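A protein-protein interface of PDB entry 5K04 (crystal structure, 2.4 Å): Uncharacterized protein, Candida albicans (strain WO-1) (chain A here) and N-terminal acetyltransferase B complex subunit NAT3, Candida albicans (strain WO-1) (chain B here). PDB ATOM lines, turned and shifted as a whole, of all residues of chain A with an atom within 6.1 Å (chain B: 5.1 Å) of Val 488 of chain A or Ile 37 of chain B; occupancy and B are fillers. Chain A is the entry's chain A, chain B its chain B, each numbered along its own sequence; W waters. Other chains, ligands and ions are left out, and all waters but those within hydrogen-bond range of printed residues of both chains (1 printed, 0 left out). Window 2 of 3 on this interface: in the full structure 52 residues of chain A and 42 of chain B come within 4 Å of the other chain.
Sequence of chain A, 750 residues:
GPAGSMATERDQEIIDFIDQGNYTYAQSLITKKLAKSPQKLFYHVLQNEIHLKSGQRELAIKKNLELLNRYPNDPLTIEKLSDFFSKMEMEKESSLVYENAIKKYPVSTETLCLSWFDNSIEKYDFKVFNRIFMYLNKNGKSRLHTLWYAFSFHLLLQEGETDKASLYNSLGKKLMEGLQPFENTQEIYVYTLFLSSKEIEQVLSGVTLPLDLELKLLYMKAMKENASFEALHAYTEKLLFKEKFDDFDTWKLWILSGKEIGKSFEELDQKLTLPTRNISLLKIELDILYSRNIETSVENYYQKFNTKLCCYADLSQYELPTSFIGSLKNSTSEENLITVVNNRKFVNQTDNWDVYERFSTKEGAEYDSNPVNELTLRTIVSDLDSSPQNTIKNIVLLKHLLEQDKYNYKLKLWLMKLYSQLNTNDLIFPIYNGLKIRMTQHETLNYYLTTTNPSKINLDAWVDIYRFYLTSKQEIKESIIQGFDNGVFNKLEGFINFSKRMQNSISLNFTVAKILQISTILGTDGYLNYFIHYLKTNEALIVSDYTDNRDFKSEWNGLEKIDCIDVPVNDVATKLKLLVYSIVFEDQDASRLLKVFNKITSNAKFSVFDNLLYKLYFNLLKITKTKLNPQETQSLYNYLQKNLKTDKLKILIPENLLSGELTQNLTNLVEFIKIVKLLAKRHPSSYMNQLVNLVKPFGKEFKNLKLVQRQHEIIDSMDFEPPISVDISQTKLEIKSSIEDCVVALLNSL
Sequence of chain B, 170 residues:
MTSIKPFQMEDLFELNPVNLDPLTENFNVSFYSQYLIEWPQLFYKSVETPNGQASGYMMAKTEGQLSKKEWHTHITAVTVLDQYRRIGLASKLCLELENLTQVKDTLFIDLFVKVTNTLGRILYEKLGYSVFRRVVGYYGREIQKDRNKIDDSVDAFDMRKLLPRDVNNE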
ATOM      1  N   GLN A 186       4.103 -20.144 -29.977  1.00  0.00           N
ATOM      2  CA  GLN A 186       4.234 -19.937 -28.534  1.00  0.00           C
ATOM      3  C   GLN A 186       4.074 -21.246 -27.769  1.00  0.00           C
ATOM      4  O   GLN A 186       4.836 -21.527 -26.831  1.00  0.00           O
ATOM      5  CB  GLN A 186       3.202 -18.916 -28.050  1.00  0.00           C
ATOM      6  CG  GLN A 186       3.385 -17.525 -28.622  1.00  0.00           C
ATOM      7  CD  GLN A 186       4.595 -16.790 -28.064  1.00  0.00           C
ATOM      8  OE1 GLN A 186       5.303 -17.276 -27.178  1.00  0.00           O
ATOM      9  NE2 GLN A 186       4.827 -15.591 -28.579  1.00  0.00           N
ATOM     10  N   GLU A 478       0.892  -4.672 -15.668  1.00  0.00           N
ATOM     11  CA  GLU A 478      -0.130  -4.866 -16.702  1.00  0.00           C
ATOM     12  C   GLU A 478       0.415  -5.656 -17.896  1.00  0.00           C
ATOM     13  O   GLU A 478      -0.274  -6.518 -18.447  1.00  0.00           O
ATOM     14  CB  GLU A 478      -0.672  -3.503 -17.153  1.00  0.00           C
ATOM     15  CG  GLU A 478      -1.818  -3.558 -18.188  1.00  0.00           C
ATOM     16  CD  GLU A 478      -3.139  -4.161 -17.653  1.00  0.00           C
ATOM     17  OE1 GLU A 478      -4.061  -4.386 -18.463  1.00  0.00           O
ATOM     18  OE2 GLU A 478      -3.252  -4.398 -16.433  1.00  0.00           O
ATOM     19  N   SER A 479       1.659  -5.384 -18.292  1.00  0.00           N
ATOM     20  CA  SER A 479       2.314  -6.162 -19.344  1.00  0.00           C
ATOM     21  C   SER A 479       2.359  -7.654 -19.000  1.00  0.00           C
ATOM     22  O   SER A 479       2.114  -8.507 -19.865  1.00  0.00           O
ATOM     23  CB  SER A 479       3.731  -5.614 -19.570  1.00  0.00           C
ATOM     24  OG  SER A 479       3.686  -4.243 -19.931  1.00  0.00           O
ATOM     25  N   ILE A 480       2.670  -7.983 -17.740  1.00  0.00           N
ATOM     26  CA  ILE A 480       2.687  -9.378 -17.302  1.00  0.00           C
ATOM     27  C   ILE A 480       1.294  -9.996 -17.376  1.00  0.00           C
ATOM     28  O   ILE A 480       1.132 -11.150 -17.787  1.00  0.00           O
ATOM     29  CB  ILE A 480       3.270  -9.477 -15.881  1.00  0.00           C
ATOM     30  CG1 ILE A 480       4.746  -9.061 -15.885  1.00  0.00           C
ATOM     31  CG2 ILE A 480       3.086 -10.885 -15.340  1.00  0.00           C
ATOM     32  CD1 ILE A 480       5.360  -8.974 -14.508  1.00  0.00           C
ATOM     33  N   GLN A 482      -1.287  -9.017 -19.328  1.00  0.00           N
ATOM     34  CA  GLN A 482      -1.672  -9.136 -20.733  1.00  0.00           C
ATOM     35  C   GLN A 482      -0.842 -10.194 -21.444  1.00  0.00           C
ATOM     36  O   GLN A 482      -1.351 -10.915 -22.311  1.00  0.00           O
ATOM     37  CB  GLN A 482      -1.508  -7.786 -21.431  1.00  0.00           C
ATOM     38  CG  GLN A 482      -2.469  -6.711 -20.979  1.00  0.00           C
ATOM     39  CD  GLN A 482      -2.119  -5.350 -21.564  1.00  0.00           C
ATOM     40  OE1 GLN A 482      -1.157  -5.214 -22.327  1.00  0.00           O
ATOM     41  NE2 GLN A 482      -2.900  -4.331 -21.206  1.00  0.00           N
ATOM     42  N   GLY A 483       0.449 -10.276 -21.118  1.00  0.00           N
ATOM     43  CA  GLY A 483       1.278 -11.303 -21.723  1.00  0.00           C
ATOM     44  C   GLY A 483       0.797 -12.702 -21.389  1.00  0.00           C
ATOM     45  O   GLY A 483       0.859 -13.597 -22.227  1.00  0.00           O
ATOM     46  N   PHE A 484       0.327 -12.915 -20.150  1.00  0.00           N
ATOM     47  CA  PHE A 484      -0.300 -14.191 -19.816  1.00  0.00           C
ATOM     48  C   PHE A 484      -1.648 -14.356 -20.518  1.00  0.00           C
ATOM     49  O   PHE A 484      -1.937 -15.427 -21.059  1.00  0.00           O
ATOM     50  CB  PHE A 484      -0.467 -14.315 -18.300  1.00  0.00           C
ATOM     51  CG  PHE A 484       0.719 -14.923 -17.586  1.00  0.00           C
ATOM     52  CD1 PHE A 484       0.850 -16.303 -17.479  1.00  0.00           C
ATOM     53  CD2 PHE A 484       1.679 -14.115 -16.990  1.00  0.00           C
ATOM     54  CE1 PHE A 484       1.923 -16.861 -16.811  1.00  0.00           C
ATOM     55  CE2 PHE A 484       2.762 -14.662 -16.322  1.00  0.00           C
ATOM     56  CZ  PHE A 484       2.889 -16.044 -16.237  1.00  0.00           C
ATOM     57  N   ASN A 486      -2.852 -13.044 -23.278  1.00  0.00           N
ATOM     58  CA  ASN A 486      -2.464 -13.501 -24.593  1.00  0.00           C
ATOM     59  C   ASN A 486      -1.605 -14.645 -25.092  1.00  0.00           C
ATOM     60  O   ASN A 486      -1.286 -14.723 -26.268  1.00  0.00           O
ATOM     61  CB  ASN A 486      -2.019 -12.313 -25.441  1.00  0.00           C
ATOM     62  CG  ASN A 486      -3.099 -11.205 -25.475  1.00  0.00           C
ATOM     63  OD1 ASN A 486      -3.990 -11.214 -26.318  1.00  0.00           O
ATOM     64  ND2 ASN A 486      -3.036 -10.282 -24.516  1.00  0.00           N
ATOM     65  N   GLY A 487      -1.146 -15.492 -24.226  1.00  0.00           N
ATOM     66  CA  GLY A 487      -0.177 -16.371 -24.862  1.00  0.00           C
ATOM     67  C   GLY A 487       1.252 -16.153 -25.272  1.00  0.00           C
ATOM     68  O   GLY A 487       1.767 -16.897 -26.105  1.00  0.00           O
ATOM     69  N   VAL A 488       1.887 -15.111 -24.731  1.00  0.00           N
ATOM     70  CA  VAL A 488       3.149 -14.632 -25.281  1.00  0.00           C
ATOM     71  C   VAL A 488       4.296 -15.115 -24.410  1.00  0.00           C
ATOM     72  O   VAL A 488       5.073 -14.320 -23.866  1.00  0.00           O
ATOM     73  CB  VAL A 488       3.141 -13.103 -25.418  1.00  0.00           C
ATOM     74  CG1 VAL A 488       4.092 -12.678 -26.518  1.00  0.00           C
ATOM     75  CG2 VAL A 488       1.727 -12.619 -25.723  1.00  0.00           C
ATOM     76  N   PHE A 489       4.419 -16.440 -24.310  1.00  0.00           N
ATOM     77  CA  PHE A 489       5.415 -17.053 -23.435  1.00  0.00           C
ATOM     78  C   PHE A 489       6.844 -16.776 -23.909  1.00  0.00           C
ATOM     79  O   PHE A 489       7.769 -16.742 -23.086  1.00  0.00           O
ATOM     80  CB  PHE A 489       5.110 -18.548 -23.340  1.00  0.00           C
ATOM     81  CG  PHE A 489       3.685 -18.834 -22.925  1.00  0.00           C
ATOM     82  CD1 PHE A 489       3.296 -18.673 -21.612  1.00  0.00           C
ATOM     83  CD2 PHE A 489       2.738 -19.218 -23.852  1.00  0.00           C
ATOM     84  CE1 PHE A 489       1.999 -18.897 -21.232  1.00  0.00           C
ATOM     85  CE2 PHE A 489       1.451 -19.452 -23.483  1.00  0.00           C
ATOM     86  CZ  PHE A 489       1.073 -19.290 -22.169  1.00  0.00           C
ATOM     87  N   ASN A 490       7.030 -16.569 -25.227  1.00  0.00           N
ATOM     88  CA  ASN A 490       8.236 -16.032 -25.877  1.00  0.00           C
ATOM     89  C   ASN A 490       8.891 -14.862 -25.150  1.00  0.00           C
ATOM     90  O   ASN A 490      10.103 -14.657 -25.263  1.00  0.00           O
ATOM     91  CB  ASN A 490       7.899 -15.538 -27.302  1.00  0.00           C
ATOM     92  CG  ASN A 490       8.211 -16.558 -28.328  1.00  0.00           C
ATOM     93  OD1 ASN A 490       8.973 -17.483 -28.065  1.00  0.00           O
ATOM     94  ND2 ASN A 490       7.644 -16.414 -29.511  1.00  0.00           N
ATOM     95  N   LYS A 491       8.078 -14.051 -24.467  1.00  0.00           N
ATOM     96  CA  LYS A 491       8.499 -12.771 -23.929  1.00  0.00           C
ATOM     97  C   LYS A 491       8.228 -12.631 -22.448  1.00  0.00           C
ATOM     98  O   LYS A 491       8.695 -11.658 -21.842  1.00  0.00           O
ATOM     99  CB  LYS A 491       7.774 -11.628 -24.657  1.00  0.00           C
ATOM    100  CG  LYS A 491       7.793 -11.714 -26.180  1.00  0.00           C
ATOM    101  CD  LYS A 491       9.222 -11.568 -26.741  1.00  0.00           C
ATOM    102  CE  LYS A 491       9.204 -11.372 -28.277  1.00  0.00           C
ATOM    103  NZ  LYS A 491      10.569 -11.503 -28.872  1.00  0.00           N
ATOM    104  N   LEU A 492       7.466 -13.563 -21.862  1.00  0.00           N
ATOM    105  CA  LEU A 492       6.954 -13.399 -20.506  1.00  0.00           C
ATOM    106  C   LEU A 492       8.078 -13.338 -19.486  1.00  0.00           C
ATOM    107  O   LEU A 492       8.098 -12.454 -18.618  1.00  0.00           O
ATOM    108  CB  LEU A 492       6.005 -14.548 -20.174  1.00  0.00           C
ATOM    109  CG  LEU A 492       4.535 -14.157 -20.221  1.00  0.00           C
ATOM    110  CD1 LEU A 492       3.646 -15.326 -19.812  1.00  0.00           C
ATOM    111  CD2 LEU A 492       4.292 -12.907 -19.336  1.00  0.00           C
ATOM    112  N   GLU A 493       9.012 -14.294 -19.565  1.00  0.00           N
ATOM    113  CA  GLU A 493      10.132 -14.329 -18.624  1.00  0.00           C
ATOM    114  C   GLU A 493      10.866 -12.996 -18.585  1.00  0.00           C
ATOM    115  O   GLU A 493      11.304 -12.553 -17.520  1.00  0.00           O
ATOM    116  CB  GLU A 493      11.088 -15.462 -19.000  1.00  0.00           C
ATOM    117  CG  GLU A 493      12.130 -15.746 -17.954  1.00  0.00           C
ATOM    118  CD  GLU A 493      12.730 -17.156 -18.053  1.00  0.00           C
ATOM    119  OE1 GLU A 493      12.516 -17.863 -19.071  1.00  0.00           O
ATOM    120  OE2 GLU A 493      13.421 -17.557 -17.093  1.00  0.00           O
ATOM    121  N   PHE A 495       9.501 -10.005 -19.268  1.00  0.00           N
ATOM    122  CA  PHE A 495       8.657  -9.060 -18.532  1.00  0.00           C
ATOM    123  C   PHE A 495       8.837  -9.241 -17.031  1.00  0.00           C
ATOM    124  O   PHE A 495       9.006  -8.272 -16.285  1.00  0.00           O
ATOM    125  CB  PHE A 495       7.179  -9.245 -18.879  1.00  0.00           C
ATOM    126  CG  PHE A 495       6.818  -8.932 -20.303  1.00  0.00           C
ATOM    127  CD1 PHE A 495       7.696  -8.268 -21.141  1.00  0.00           C
ATOM    128  CD2 PHE A 495       5.581  -9.304 -20.796  1.00  0.00           C
ATOM    129  CE1 PHE A 495       7.348  -7.986 -22.445  1.00  0.00           C
ATOM    130  CE2 PHE A 495       5.226  -9.024 -22.112  1.00  0.00           C
ATOM    131  CZ  PHE A 495       6.110  -8.367 -22.933  1.00  0.00           C
ATOM    132  N   SER B  33       6.426  -2.987 -24.426  1.00  0.00           N
ATOM    133  CA  SER B  33       5.833  -4.264 -24.048  1.00  0.00           C
ATOM    134  C   SER B  33       4.586  -4.566 -24.878  1.00  0.00           C
ATOM    135  O   SER B  33       4.293  -5.735 -25.157  1.00  0.00           O
ATOM    136  CB  SER B  33       5.497  -4.256 -22.556  1.00  0.00           C
ATOM    137  OG  SER B  33       4.415  -3.370 -22.325  1.00  0.00           O
ATOM    138  N   GLN B  34       3.847  -3.526 -25.267  1.00  0.00           N
ATOM    139  CA  GLN B  34       2.684  -3.691 -26.136  1.00  0.00           C
ATOM    140  C   GLN B  34       3.073  -4.290 -27.481  1.00  0.00           C
ATOM    141  O   GLN B  34       2.379  -5.167 -28.003  1.00  0.00           O
ATOM    142  CB  GLN B  34       1.984  -2.336 -26.350  1.00  0.00           C
ATOM    143  CG  GLN B  34       0.805  -2.400 -27.324  1.00  0.00           C
ATOM    144  CD  GLN B  34       0.304  -1.028 -27.817  1.00  0.00           C
ATOM    145  OE1 GLN B  34       1.049  -0.046 -27.886  1.00  0.00           O
ATOM    146  NE2 GLN B  34      -0.973  -0.975 -28.167  1.00  0.00           N
ATOM    147  N   TYR B  35       4.163  -3.799 -28.077  1.00  0.00           N
ATOM    148  CA  TYR B  35       4.620  -4.371 -29.338  1.00  0.00           C
ATOM    149  C   TYR B  35       5.070  -5.812 -29.159  1.00  0.00           C
ATOM    150  O   TYR B  35       4.791  -6.664 -30.009  1.00  0.00           O
ATOM    151  CB  TYR B  35       5.734  -3.506 -29.922  1.00  0.00           C
ATOM    152  CG  TYR B  35       5.168  -2.337 -30.698  1.00  0.00           C
ATOM    153  CD1 TYR B  35       4.419  -1.353 -30.059  1.00  0.00           C
ATOM    154  CD2 TYR B  35       5.364  -2.225 -32.064  1.00  0.00           C
ATOM    155  CE1 TYR B  35       3.886  -0.278 -30.765  1.00  0.00           C
ATOM    156  CE2 TYR B  35       4.840  -1.164 -32.780  1.00  0.00           C
ATOM    157  CZ  TYR B  35       4.105  -0.198 -32.126  1.00  0.00           C
ATOM    158  OH  TYR B  35       3.576   0.838 -32.836  1.00  0.00           O
ATOM    159  N   LEU B  36       5.748  -6.109 -28.045  1.00  0.00           N
ATOM    160  CA  LEU B  36       6.130  -7.489 -27.768  1.00  0.00           C
ATOM    161  C   LEU B  36       4.919  -8.368 -27.501  1.00  0.00           C
ATOM    162  O   LEU B  36       4.975  -9.576 -27.747  1.00  0.00           O
ATOM    163  CB  LEU B  36       7.085  -7.556 -26.580  1.00  0.00           C
ATOM    164  CG  LEU B  36       8.429  -6.867 -26.827  1.00  0.00           C
ATOM    165  CD1 LEU B  36       9.165  -6.727 -25.516  1.00  0.00           C
ATOM    166  CD2 LEU B  36       9.293  -7.610 -27.841  1.00  0.00           C
ATOM    167  N   ILE B  37       3.819  -7.787 -27.009  1.00  0.00           N
ATOM    168  CA  ILE B  37       2.638  -8.589 -26.704  1.00  0.00           C
ATOM    169  C   ILE B  37       1.838  -8.863 -27.972  1.00  0.00           C
ATOM    170  O   ILE B  37       1.448 -10.007 -28.236  1.00  0.00           O
ATOM    171  CB  ILE B  37       1.788  -7.899 -25.615  1.00  0.00           C
ATOM    172  CG1 ILE B  37       2.404  -8.135 -24.231  1.00  0.00           C
ATOM    173  CG2 ILE B  37       0.338  -8.407 -25.625  1.00  0.00           C
ATOM    174  CD1 ILE B  37       2.020  -7.077 -23.224  1.00  0.00           C
ATOM    175  N   GLU B  38       1.629  -7.827 -28.798  1.00  0.00           N
ATOM    176  CA  GLU B  38       0.718  -7.907 -29.938  1.00  0.00           C
ATOM    177  C   GLU B  38       1.401  -8.357 -31.228  1.00  0.00           C
ATOM    178  O   GLU B  38       0.833  -9.161 -31.974  1.00  0.00           O
ATOM    179  CB  GLU B  38       0.013  -6.561 -30.134  1.00  0.00           C
ATOM    180  CG  GLU B  38      -1.133  -6.348 -29.125  1.00  0.00           C
ATOM    181  CD  GLU B  38      -1.902  -5.068 -29.343  1.00  0.00           C
ATOM    182  OE1 GLU B  38      -2.385  -4.847 -30.472  1.00  0.00           O
ATOM    183  OE2 GLU B  38      -2.031  -4.279 -28.379  1.00  0.00           O
ATOM    184  N   TRP B  39       2.617  -7.889 -31.504  1.00  0.00           N
ATOM    185  CA  TRP B  39       3.359  -8.281 -32.703  1.00  0.00           C
ATOM    186  C   TRP B  39       4.772  -8.679 -32.302  1.00  0.00           C
ATOM    187  O   TRP B  39       5.750  -8.023 -32.680  1.00  0.00           O
ATOM    188  CB  TRP B  39       3.372  -7.154 -33.739  1.00  0.00           C
ATOM    189  CG  TRP B  39       2.044  -6.489 -33.842  1.00  0.00           C
ATOM    190  CD1 TRP B  39       0.976  -6.895 -34.594  1.00  0.00           C
ATOM    191  CD2 TRP B  39       1.619  -5.309 -33.141  1.00  0.00           C
ATOM    192  NE1 TRP B  39      -0.090  -6.044 -34.401  1.00  0.00           N
ATOM    193  CE2 TRP B  39       0.277  -5.060 -33.517  1.00  0.00           C
ATOM    194  CE3 TRP B  39       2.241  -4.446 -32.224  1.00  0.00           C
ATOM    195  CZ2 TRP B  39      -0.457  -3.977 -33.014  1.00  0.00           C
ATOM    196  CZ3 TRP B  39       1.516  -3.359 -31.729  1.00  0.00           C
ATOM    197  CH2 TRP B  39       0.176  -3.143 -32.120  1.00  0.00           C
ATOM    198  N   PRO B  40       4.914  -9.780 -31.554  1.00  0.00           N
ATOM    199  CA  PRO B  40       6.245 -10.136 -31.021  1.00  0.00           C
ATOM    200  C   PRO B  40       7.290 -10.434 -32.082  1.00  0.00           C
ATOM    201  O   PRO B  40       8.485 -10.215 -31.830  1.00  0.00           O
ATOM    202  CB  PRO B  40       5.965 -11.372 -30.152  1.00  0.00           C
ATOM    203  CG  PRO B  40       4.583 -11.841 -30.525  1.00  0.00           C
ATOM    204  CD  PRO B  40       3.841 -10.674 -31.065  1.00  0.00           C
HETATM  205  O   HOH W   1      10.953 -10.775 -31.520  1.00  0.00           O
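The side-chain hydroxyl of Ser 33 of chain B is in hydrogen-bond range of the side-chain hydroxyl of Ser 479 of chain A, at 2.7 Å.
The backbone carbonyl oxygen (O) of Gln 482 of chain A is in hydrogen-bond range of the side-chain amide nitrogen (ND2) of Asn 486 of chain A (2.8 Å).
O of Gly 483 of chain A sits at hydrogen-bond distance from N of Val 488 of chain A, 3.1 Å away.
The side-chain carboxylate (OE1) of Glu 478 of chain A lies within hydrogen-bond range of the side-chain amide nitrogen (NE2) of Gln 482 of chain A, 3.0 Å away.
Among the printed residues, merely in contact across the chains: Ser 479 of chain A with Ile 37 of chain B, Gln 482 of chain A with Ile 37 of chain B, Val 488 of chain A with Leu 36 of chain B, Val 488 of chain A with Ile 37 of chain B, Lys 491 of chain A with Leu 36 of chain B, Lys 491 of chain A with Pro 40 of chain B, Phe 495 of chain A with Ser 33 of chain B, Phe 495 of chain A with Leu 36 of chain B and Phe 495 of chain A with Ile 37 of chain B.
Of the printed residues of chain B, Gln 482 of chain A touches Ile 37 (3.8 Å).
Phe 484 of chain A touches none of the printed residues of chain B.
Of chain B, only Leu 36 and Ile 37 come within 4 Å of Val 488 of chain A.
Of the printed residues of chain A, Leu 36 of chain B touches Val 488, Lys 491 and Phe 495.
Printed residues of chain A within 4 Å of Ile 37 of chain B: Ser 479 (3.7 Å), Gln 482 (3.8 Å), Val 488 (3.6 Å) and Phe 495 (3.6 Å).
The nearest residue of chain B that does not touch Val 488 of chain A is Pro 40 of chain B (4.1 Å).
Hydrophobic or aromatic side chains of chain A that line the printed part of chain B: Val 488 and Phe 495.
Hydrophobic or aromatic side chains of chain B that line the printed part of chain A: Leu 36, Ile 37 and Pro 40.
Along chain B the printed residues that touch a printed residue of chain A span positions 33 to 40.
Among the printed residues, no Asp or Glu carboxylate lies within 4 Å of a Lys or Arg side-chain nitrogen of the other chain.
Water W1 lies within hydrogen-bond range of O of Pro 40 of chain B and NZ of Lys 491 of chain A.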
